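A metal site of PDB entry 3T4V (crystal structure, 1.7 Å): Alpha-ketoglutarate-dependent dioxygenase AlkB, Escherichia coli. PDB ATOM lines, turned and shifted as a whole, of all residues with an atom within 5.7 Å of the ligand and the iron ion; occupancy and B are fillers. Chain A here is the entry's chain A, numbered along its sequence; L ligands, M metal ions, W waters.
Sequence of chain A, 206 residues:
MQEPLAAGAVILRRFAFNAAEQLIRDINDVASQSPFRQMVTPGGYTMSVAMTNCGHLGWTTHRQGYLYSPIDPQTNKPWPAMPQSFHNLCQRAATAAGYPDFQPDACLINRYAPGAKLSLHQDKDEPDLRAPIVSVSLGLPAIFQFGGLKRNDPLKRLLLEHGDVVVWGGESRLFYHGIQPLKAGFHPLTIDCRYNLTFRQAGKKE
O2 of the ligand lies within hydrogen-bond range of OH of Tyr 112 (2.6 Å).
O1 of the ligand lies within salt-bridge range of NH2 of Arg 200 (2.9 Å).
OD1 of Asn 196 lies close to O2 of the ligand, 3.5 Å away.
OG1 of Thr 198 lies within hydrogen-bond range of O1 of the ligand, at 3.3 Å.
O3 of the ligand is in salt-bridge range of NH1 of Arg 194, at 2.7 Å.
OD1 of Asn 110 sits close to O2 of the ligand (2.9 Å).
A ring nitrogen (ND1) of His 177 lies within hydrogen-bond range of the backbone carbonyl oxygen of Phe 175 (2.9 Å).
N of Asn 196 is in hydrogen-bond range of O of Asn 110 (2.9 Å).
The backbone carbonyl oxygen (O) of Ile 133 lies within hydrogen-bond range of the backbone NH (N) of Trp 168, at 2.8 Å.
The indole nitrogen (NE1) of Trp 168 lies within hydrogen-bond range of the side-chain hydroxyl (OG) of Ser 135 (2.9 Å).
The guanidinium group (NH2) of Arg 194 sits close to the side-chain amide nitrogen (ND2) of Asn 196, 3.3 Å away.
OD2 of Asp 123 is in salt-bridge range of NH1 of Arg 200 (3.0 Å).
The backbone NH (N) of Ile 179 lies within hydrogen-bond range of the backbone carbonyl oxygen (O) of Leu 118.
O of Asp 123 sits at hydrogen-bond distance from NH1 of Arg 173 (2.9 Å).
Leu 108 touches the ligand (CD2 to O1, 3.9 Å).
CD2 of Leu 118 touches O4 of the ligand, 3.6 Å away.
CD1 of Ile 133 touches C14 of the ligand (3.6 Å).
Ser 135 touches the ligand.
Phe 144 touches the ligand (CE1 to C7, 3.6 Å).
Trp 168 touches the ligand (CE2 to C12, 3.2 Å).
O of Ser 172 touches C16 of the ligand (3.5 Å).
O of Arg 173 touches C15 of the ligand (3.4 Å).
Ile 179 touches the ligand (CG1 to O3, 3.4 Å).
Hydrophobic or aromatic side chains that line the ligand: Leu 108, Tyr 112, Leu 118, His 121, Ile 133, Phe 144, Trp 168, His 177 and Ile 179.
Of the 24 residues printed, 18 come within 4 Å of the ligand.
The nearest printed residue that does not touch the ligand is Leu 160 (4.2 Å).
The nearest printed residue that does not touch the iron ion is Arg 200 (4.7 Å).
The iron ion is bound by a ring nitrogen (NE2) of His 177 (2.1 Å).
O5 of the ligand binds the iron ion (2.1 Å).
OD1 of Asp 123 is bound to the iron ion (2.1 Å).
A ring nitrogen (NE2) of His 121 is bound to the iron ion (2.1 Å).
An oxygen (O4) of the ligand binds the iron ion (2.2 Å).
The iron ion has five donor atoms within binding distance.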
ATOM      1  N   LEU A 108      13.301  -5.781   9.942  1.00  0.00           N
ATOM      2  CA  LEU A 108      12.710  -6.673   8.935  1.00  0.00           C
ATOM      3  C   LEU A 108      11.955  -5.805   7.947  1.00  0.00           C
ATOM      4  O   LEU A 108      11.219  -4.917   8.355  1.00  0.00           O
ATOM      5  CB  LEU A 108      11.733  -7.660   9.594  1.00  0.00           C
ATOM      6  CG  LEU A 108      10.922  -8.590   8.685  1.00  0.00           C
ATOM      7  CD1 LEU A 108      11.857  -9.528   7.979  1.00  0.00           C
ATOM      8  CD2 LEU A 108       9.918  -9.420   9.522  1.00  0.00           C
ATOM      9  N   ASN A 110       9.303  -5.866   5.027  1.00  0.00           N
ATOM     10  CA  ASN A 110       8.217  -6.644   4.396  1.00  0.00           C
ATOM     11  C   ASN A 110       7.730  -5.925   3.141  1.00  0.00           C
ATOM     12  O   ASN A 110       7.387  -4.744   3.198  1.00  0.00           O
ATOM     13  CB  ASN A 110       7.030  -6.792   5.370  1.00  0.00           C
ATOM     14  CG  ASN A 110       7.297  -7.784   6.504  1.00  0.00           C
ATOM     15  OD1 ASN A 110       6.530  -7.855   7.507  1.00  0.00           O
ATOM     16  ND2 ASN A 110       8.339  -8.551   6.373  1.00  0.00           N
ATOM     17  N   TYR A 112       4.734  -6.026   0.226  1.00  0.00           N
ATOM     18  CA  TYR A 112       3.401  -6.503  -0.194  1.00  0.00           C
ATOM     19  C   TYR A 112       3.068  -6.108  -1.616  1.00  0.00           C
ATOM     20  O   TYR A 112       2.843  -4.917  -1.904  1.00  0.00           O
ATOM     21  CB  TYR A 112       2.287  -5.881   0.691  1.00  0.00           C
ATOM     22  CG  TYR A 112       2.453  -6.304   2.141  1.00  0.00           C
ATOM     23  CD1 TYR A 112       3.415  -5.737   2.954  1.00  0.00           C
ATOM     24  CD2 TYR A 112       1.610  -7.275   2.701  1.00  0.00           C
ATOM     25  CE1 TYR A 112       3.578  -6.142   4.285  1.00  0.00           C
ATOM     26  CE2 TYR A 112       1.776  -7.698   4.020  1.00  0.00           C
ATOM     27  CZ  TYR A 112       2.757  -7.114   4.799  1.00  0.00           C
ATOM     28  OH  TYR A 112       2.911  -7.529   6.085  1.00  0.00           O
ATOM     29  N   LEU A 118      -0.444 -11.052   5.767  1.00  0.00           N
ATOM     30  CA  LEU A 118       0.365 -11.615   6.812  1.00  0.00           C
ATOM     31  C   LEU A 118      -0.604 -12.153   7.861  1.00  0.00           C
ATOM     32  O   LEU A 118      -1.404 -11.408   8.431  1.00  0.00           O
ATOM     33  CB  LEU A 118       1.278 -10.535   7.391  1.00  0.00           C
ATOM     34  CG  LEU A 118       2.468 -10.999   8.211  1.00  0.00           C
ATOM     35  CD1 LEU A 118       3.423 -11.854   7.345  1.00  0.00           C
ATOM     36  CD2 LEU A 118       3.171  -9.796   8.775  1.00  0.00           C
ATOM     37  N   HIS A 121      -0.503 -13.441  14.055  1.00  0.00           N
ATOM     38  CA  HIS A 121       0.629 -13.990  14.801  1.00  0.00           C
ATOM     39  C   HIS A 121       0.990 -13.024  15.914  1.00  0.00           C
ATOM     40  O   HIS A 121       0.522 -11.879  15.941  1.00  0.00           O
ATOM     41  CB  HIS A 121       1.841 -14.154  13.896  1.00  0.00           C
ATOM     42  CG  HIS A 121       2.379 -12.850  13.404  1.00  0.00           C
ATOM     43  ND1 HIS A 121       1.801 -12.178  12.344  1.00  0.00           N
ATOM     44  CD2 HIS A 121       3.379 -12.070  13.856  1.00  0.00           C
ATOM     45  CE1 HIS A 121       2.446 -11.035  12.160  1.00  0.00           C
ATOM     46  NE2 HIS A 121       3.399 -10.949  13.061  1.00  0.00           N
ATOM     47  N   GLN A 122       1.817 -13.514  16.841  1.00  0.00           N
ATOM     48  CA  GLN A 122       2.513 -12.695  17.830  1.00  0.00           C
ATOM     49  C   GLN A 122       3.965 -12.623  17.431  1.00  0.00           C
ATOM     50  O   GLN A 122       4.506 -13.562  16.819  1.00  0.00           O
ATOM     51  CB  GLN A 122       2.420 -13.343  19.218  1.00  0.00           C
ATOM     52  CG  GLN A 122       1.034 -13.298  19.819  1.00  0.00           C
ATOM     53  CD  GLN A 122       0.994 -13.967  21.167  1.00  0.00           C
ATOM     54  OE1 GLN A 122       1.285 -15.152  21.278  1.00  0.00           O
ATOM     55  NE2 GLN A 122       0.656 -13.208  22.210  1.00  0.00           N
ATOM     56  N   ASP A 123       4.642 -11.529  17.804  1.00  0.00           N
ATOM     57  CA  ASP A 123       6.075 -11.564  17.693  1.00  0.00           C
ATOM     58  C   ASP A 123       6.596 -11.845  19.084  1.00  0.00           C
ATOM     59  O   ASP A 123       6.603 -10.986  19.980  1.00  0.00           O
ATOM     60  CB  ASP A 123       6.530 -10.184  17.247  1.00  0.00           C
ATOM     61  CG  ASP A 123       6.284  -9.968  15.774  1.00  0.00           C
ATOM     62  OD1 ASP A 123       5.141  -9.637  15.437  1.00  0.00           O
ATOM     63  OD2 ASP A 123       7.231 -10.140  14.978  1.00  0.00           O
ATOM     64  N   ILE A 133       8.459  -2.829  19.510  1.00  0.00           N
ATOM     65  CA  ILE A 133       8.792  -2.895  18.104  1.00  0.00           C
ATOM     66  C   ILE A 133       8.269  -1.641  17.453  1.00  0.00           C
ATOM     67  O   ILE A 133       7.149  -1.191  17.777  1.00  0.00           O
ATOM     68  CB  ILE A 133       8.239  -4.198  17.452  1.00  0.00           C
ATOM     69  CG1 ILE A 133       9.037  -5.425  17.948  1.00  0.00           C
ATOM     70  CG2 ILE A 133       8.253  -4.138  15.897  1.00  0.00           C
ATOM     71  CD1 ILE A 133       8.508  -6.809  17.488  1.00  0.00           C
ATOM     72  N   SER A 135       7.060   0.022  13.858  1.00  0.00           N
ATOM     73  CA  SER A 135       6.749  -0.202  12.444  1.00  0.00           C
ATOM     74  C   SER A 135       6.641   1.106  11.677  1.00  0.00           C
ATOM     75  O   SER A 135       6.195   2.138  12.219  1.00  0.00           O
ATOM     76  CB  SER A 135       5.411  -0.970  12.269  1.00  0.00           C
ATOM     77  OG  SER A 135       4.330  -0.211  12.805  1.00  0.00           O
ATOM     78  N   SER A 137       5.199   2.297   7.834  1.00  0.00           N
ATOM     79  CA  SER A 137       4.447   1.847   6.651  1.00  0.00           C
ATOM     80  C   SER A 137       4.683   2.840   5.525  1.00  0.00           C
ATOM     81  O   SER A 137       4.711   4.051   5.740  1.00  0.00           O
ATOM     82  CB  SER A 137       2.949   1.734   6.957  1.00  0.00           C
ATOM     83  OG  SER A 137       2.721   0.745   7.957  1.00  0.00           O
ATOM     84  N   PHE A 144      -4.674  -3.282   8.952  1.00  0.00           N
ATOM     85  CA  PHE A 144      -4.016  -3.984  10.053  1.00  0.00           C
ATOM     86  C   PHE A 144      -5.042  -4.516  11.037  1.00  0.00           C
ATOM     87  O   PHE A 144      -5.947  -3.787  11.487  1.00  0.00           O
ATOM     88  CB  PHE A 144      -3.056  -2.982  10.721  1.00  0.00           C
ATOM     89  CG  PHE A 144      -2.418  -3.470  12.001  1.00  0.00           C
ATOM     90  CD1 PHE A 144      -1.352  -4.376  11.966  1.00  0.00           C
ATOM     91  CD2 PHE A 144      -2.860  -2.986  13.223  1.00  0.00           C
ATOM     92  CE1 PHE A 144      -0.752  -4.810  13.142  1.00  0.00           C
ATOM     93  CE2 PHE A 144      -2.266  -3.414  14.404  1.00  0.00           C
ATOM     94  CZ  PHE A 144      -1.217  -4.333  14.369  1.00  0.00           C
ATOM     95  N   LEU A 160      -3.330   1.306   7.915  1.00  0.00           N
ATOM     96  CA  LEU A 160      -1.985   1.862   8.042  1.00  0.00           C
ATOM     97  C   LEU A 160      -1.668   2.474   6.677  1.00  0.00           C
ATOM     98  O   LEU A 160      -1.753   1.801   5.647  1.00  0.00           O
ATOM     99  CB  LEU A 160      -0.965   0.796   8.435  1.00  0.00           C
ATOM    100  CG  LEU A 160      -1.174   0.267   9.868  1.00  0.00           C
ATOM    101  CD1 LEU A 160      -0.256  -0.917  10.112  1.00  0.00           C
ATOM    102  CD2 LEU A 160      -0.894   1.381  10.919  1.00  0.00           C
ATOM    103  N   TRP A 168       4.998  -0.079  19.155  1.00  0.00           N
ATOM    104  CA  TRP A 168       4.139  -1.029  19.832  1.00  0.00           C
ATOM    105  C   TRP A 168       4.828  -1.426  21.141  1.00  0.00           C
ATOM    106  O   TRP A 168       5.717  -2.285  21.179  1.00  0.00           O
ATOM    107  CB  TRP A 168       4.027  -2.257  18.879  1.00  0.00           C
ATOM    108  CG  TRP A 168       3.477  -1.914  17.510  1.00  0.00           C
ATOM    109  CD1 TRP A 168       4.182  -1.650  16.356  1.00  0.00           C
ATOM    110  CD2 TRP A 168       2.104  -1.753  17.174  1.00  0.00           C
ATOM    111  NE1 TRP A 168       3.311  -1.339  15.322  1.00  0.00           N
ATOM    112  CE2 TRP A 168       2.025  -1.388  15.808  1.00  0.00           C
ATOM    113  CE3 TRP A 168       0.911  -1.868  17.919  1.00  0.00           C
ATOM    114  CZ2 TRP A 168       0.813  -1.167  15.165  1.00  0.00           C
ATOM    115  CZ3 TRP A 168      -0.288  -1.649  17.277  1.00  0.00           C
ATOM    116  CH2 TRP A 168      -0.340  -1.297  15.918  1.00  0.00           C
ATOM    117  N   SER A 172       0.363  -3.870  24.006  1.00  0.00           N
ATOM    118  CA  SER A 172       0.156  -4.060  22.594  1.00  0.00           C
ATOM    119  C   SER A 172       1.304  -4.838  21.984  1.00  0.00           C
ATOM    120  O   SER A 172       1.138  -5.457  20.917  1.00  0.00           O
ATOM    121  CB  SER A 172       0.006  -2.710  21.869  1.00  0.00           C
ATOM    122  OG  SER A 172       1.275  -2.108  21.668  1.00  0.00           O
ATOM    123  N   ARG A 173       2.461  -4.784  22.636  1.00  0.00           N
ATOM    124  CA  ARG A 173       3.641  -5.495  22.122  1.00  0.00           C
ATOM    125  C   ARG A 173       3.358  -7.003  21.966  1.00  0.00           C
ATOM    126  O   ARG A 173       3.953  -7.693  21.102  1.00  0.00           O
ATOM    127  CB  ARG A 173       4.799  -5.225  23.088  1.00  0.00           C
ATOM    128  CG  ARG A 173       6.072  -6.001  22.833  1.00  0.00           C
ATOM    129  CD  ARG A 173       6.757  -5.583  21.533  1.00  0.00           C
ATOM    130  NE  ARG A 173       7.975  -6.375  21.414  1.00  0.00           N
ATOM    131  CZ  ARG A 173       7.979  -7.606  20.917  1.00  0.00           C
ATOM    132  NH1 ARG A 173       6.832  -8.123  20.477  1.00  0.00           N
ATOM    133  NH2 ARG A 173       9.107  -8.291  20.828  1.00  0.00           N
ATOM    134  N   LEU A 174       2.445  -7.522  22.798  1.00  0.00           N
ATOM    135  CA  LEU A 174       2.074  -8.942  22.816  1.00  0.00           C
ATOM    136  C   LEU A 174       0.819  -9.311  22.035  1.00  0.00           C
ATOM    137  O   LEU A 174       0.385 -10.456  22.107  1.00  0.00           O
ATOM    138  CB  LEU A 174       1.870  -9.448  24.240  1.00  0.00           C
ATOM    139  CG  LEU A 174       3.082  -9.408  25.154  1.00  0.00           C
ATOM    140  CD1 LEU A 174       2.843 -10.296  26.357  1.00  0.00           C
ATOM    141  CD2 LEU A 174       4.322  -9.841  24.394  1.00  0.00           C
ATOM    142  N   PHE A 175       0.182  -8.344  21.389  1.00  0.00           N
ATOM    143  CA  PHE A 175      -1.111  -8.626  20.752  1.00  0.00           C
ATOM    144  C   PHE A 175      -0.889  -9.530  19.541  1.00  0.00           C
ATOM    145  O   PHE A 175       0.118  -9.404  18.822  1.00  0.00           O
ATOM    146  CB  PHE A 175      -1.764  -7.340  20.220  1.00  0.00           C
ATOM    147  CG  PHE A 175      -2.438  -6.498  21.275  1.00  0.00           C
ATOM    148  CD1 PHE A 175      -2.954  -5.250  20.930  1.00  0.00           C
ATOM    149  CD2 PHE A 175      -2.541  -6.921  22.576  1.00  0.00           C
ATOM    150  CE1 PHE A 175      -3.587  -4.446  21.884  1.00  0.00           C
ATOM    151  CE2 PHE A 175      -3.161  -6.126  23.539  1.00  0.00           C
ATOM    152  CZ  PHE A 175      -3.692  -4.876  23.170  1.00  0.00           C
ATOM    153  N   HIS A 177      -1.662 -10.066  15.754  1.00  0.00           N
ATOM    154  CA  HIS A 177      -1.908  -9.020  14.754  1.00  0.00           C
ATOM    155  C   HIS A 177      -1.567  -9.586  13.392  1.00  0.00           C
ATOM    156  O   HIS A 177      -0.906 -10.633  13.290  1.00  0.00           O
ATOM    157  CB  HIS A 177      -1.065  -7.780  15.053  1.00  0.00           C
ATOM    158  CG  HIS A 177       0.408  -8.069  15.074  1.00  0.00           C
ATOM    159  ND1 HIS A 177       1.033  -8.608  16.177  1.00  0.00           N
ATOM    160  CD2 HIS A 177       1.343  -7.996  14.097  1.00  0.00           C
ATOM    161  CE1 HIS A 177       2.307  -8.815  15.886  1.00  0.00           C
ATOM    162  NE2 HIS A 177       2.513  -8.450  14.635  1.00  0.00           N
ATOM    163  N   GLY A 178      -2.001  -8.889  12.334  1.00  0.00           N
ATOM    164  CA  GLY A 178      -1.688  -9.305  10.979  1.00  0.00           C
ATOM    165  C   GLY A 178      -2.114  -8.251   9.968  1.00  0.00           C
ATOM    166  O   GLY A 178      -2.601  -7.181  10.325  1.00  0.00           O
ATOM    167  N   ILE A 179      -1.959  -8.565   8.688  1.00  0.00           N
ATOM    168  CA  ILE A 179      -2.273  -7.619   7.602  1.00  0.00           C
ATOM    169  C   ILE A 179      -3.187  -8.377   6.629  1.00  0.00           C
ATOM    170  O   ILE A 179      -2.883  -9.510   6.240  1.00  0.00           O
ATOM    171  CB  ILE A 179      -1.007  -7.176   6.872  1.00  0.00           C
ATOM    172  CG1 ILE A 179      -0.148  -6.317   7.804  1.00  0.00           C
ATOM    173  CG2 ILE A 179      -1.333  -6.397   5.572  1.00  0.00           C
ATOM    174  CD1 ILE A 179      -0.731  -4.866   8.040  1.00  0.00           C
ATOM    175  N   ARG A 194       3.301  -2.102  -1.093  1.00  0.00           N
ATOM    176  CA  ARG A 194       3.506  -1.535   0.234  1.00  0.00           C
ATOM    177  C   ARG A 194       4.792  -2.080   0.852  1.00  0.00           C
ATOM    178  O   ARG A 194       5.130  -3.254   0.668  1.00  0.00           O
ATOM    179  CB  ARG A 194       2.306  -1.916   1.120  1.00  0.00           C
ATOM    180  CG  ARG A 194       2.489  -1.557   2.611  1.00  0.00           C
ATOM    181  CD  ARG A 194       1.166  -1.816   3.400  1.00  0.00           C
ATOM    182  NE  ARG A 194       1.334  -1.463   4.802  1.00  0.00           N
ATOM    183  CZ  ARG A 194       1.668  -2.299   5.781  1.00  0.00           C
ATOM    184  NH1 ARG A 194       1.880  -3.600   5.534  1.00  0.00           N
ATOM    185  NH2 ARG A 194       1.814  -1.823   7.018  1.00  0.00           N
ATOM    186  N   ASN A 196       6.802  -2.352   4.679  1.00  0.00           N
ATOM    187  CA  ASN A 196       6.700  -2.115   6.109  1.00  0.00           C
ATOM    188  C   ASN A 196       8.031  -2.449   6.770  1.00  0.00           C
ATOM    189  O   ASN A 196       8.574  -3.531   6.568  1.00  0.00           O
ATOM    190  CB  ASN A 196       5.588  -2.939   6.755  1.00  0.00           C
ATOM    191  CG  ASN A 196       5.421  -2.614   8.206  1.00  0.00           C
ATOM    192  OD1 ASN A 196       5.943  -3.305   9.067  1.00  0.00           O
ATOM    193  ND2 ASN A 196       4.715  -1.542   8.484  1.00  0.00           N
ATOM    194  N   THR A 198       9.994  -3.116  10.283  1.00  0.00           N
ATOM    195  CA  THR A 198       9.842  -3.294  11.743  1.00  0.00           C
ATOM    196  C   THR A 198      11.195  -3.418  12.420  1.00  0.00           C
ATOM    197  O   THR A 198      11.977  -4.324  12.139  1.00  0.00           O
ATOM    198  CB  THR A 198       8.976  -4.510  12.145  1.00  0.00           C
ATOM    199  OG1 THR A 198       9.385  -5.661  11.392  1.00  0.00           O
ATOM    200  CG2 THR A 198       7.496  -4.252  11.913  1.00  0.00           C
ATOM    201  N   ARG A 200      13.481  -4.046  15.638  1.00  0.00           N
ATOM    202  CA  ARG A 200      13.456  -4.952  16.816  1.00  0.00           C
ATOM    203  C   ARG A 200      14.779  -4.929  17.557  1.00  0.00           C
ATOM    204  O   ARG A 200      15.817  -4.795  16.920  1.00  0.00           O
ATOM    205  CB  ARG A 200      13.241  -6.391  16.309  1.00  0.00           C
ATOM    206  CG  ARG A 200      11.922  -6.572  15.518  1.00  0.00           C
ATOM    207  CD  ARG A 200      12.138  -7.203  14.156  1.00  0.00           C
ATOM    208  NE  ARG A 200      10.877  -7.236  13.394  1.00  0.00           N
ATOM    209  CZ  ARG A 200       9.862  -8.051  13.692  1.00  0.00           C
ATOM    210  NH1 ARG A 200       9.963  -8.887  14.730  1.00  0.00           N
ATOM    211  NH2 ARG A 200       8.736  -8.009  12.974  1.00  0.00           N
HETATM  212  C1  LIG L   1       2.488  -5.319  17.093  1.00  0.00           C
HETATM  213  N1  LIG L   1       4.343  -6.623  10.217  1.00  0.00           N
HETATM  214  O1  LIG L   1       6.756  -7.619  10.916  1.00  0.00           O
HETATM  215  S1  LIG L   1       2.867  -3.561  10.850  1.00  0.00           S
HETATM  216  C2  LIG L   1       5.812  -7.997  11.664  1.00  0.00           C
HETATM  217  O2  LIG L   1       4.306  -6.030   7.656  1.00  0.00           O
HETATM  218  C3  LIG L   1       4.448  -7.560  11.276  1.00  0.00           C
HETATM  219  O3  LIG L   1       2.746  -4.552   7.938  1.00  0.00           O
HETATM  220  C4  LIG L   1       3.106  -6.146   9.696  1.00  0.00           C
HETATM  221  O4  LIG L   1       3.494  -8.010  11.836  1.00  0.00           O
HETATM  222  C5  LIG L   1       3.394  -5.531   8.364  1.00  0.00           C
HETATM  223  O5  LIG L   1       5.992  -8.747  12.674  1.00  0.00           O
HETATM  224  C6  LIG L   1       2.312  -5.229  10.565  1.00  0.00           C
HETATM  225  C7  LIG L   1       2.475  -3.349  12.566  1.00  0.00           C
HETATM  226  C8  LIG L   1       3.137  -4.185  13.619  1.00  0.00           C
HETATM  227  C9  LIG L   1       4.391  -4.740  13.404  1.00  0.00           C
HETATM  228  C10 LIG L   1       4.997  -5.475  14.417  1.00  0.00           C
HETATM  229  C11 LIG L   1       4.373  -5.678  15.645  1.00  0.00           C
HETATM  230  C12 LIG L   1       2.502  -4.368  14.847  1.00  0.00           C
HETATM  231  C13 LIG L   1       3.121  -5.112  15.868  1.00  0.00           C
HETATM  232  C14 LIG L   1       4.986  -6.445  16.651  1.00  0.00           C
HETATM  233  C15 LIG L   1       4.360  -6.625  17.883  1.00  0.00           C
HETATM  234  C16 LIG L   1       3.083  -6.070  18.094  1.00  0.00           C
HETATM  235 FE    FE M   1       4.196  -9.067  13.638  1.00  0.00          FE
HETATM  236  O   HOH W   1       8.132  -5.484   8.954  1.00  0.00           O
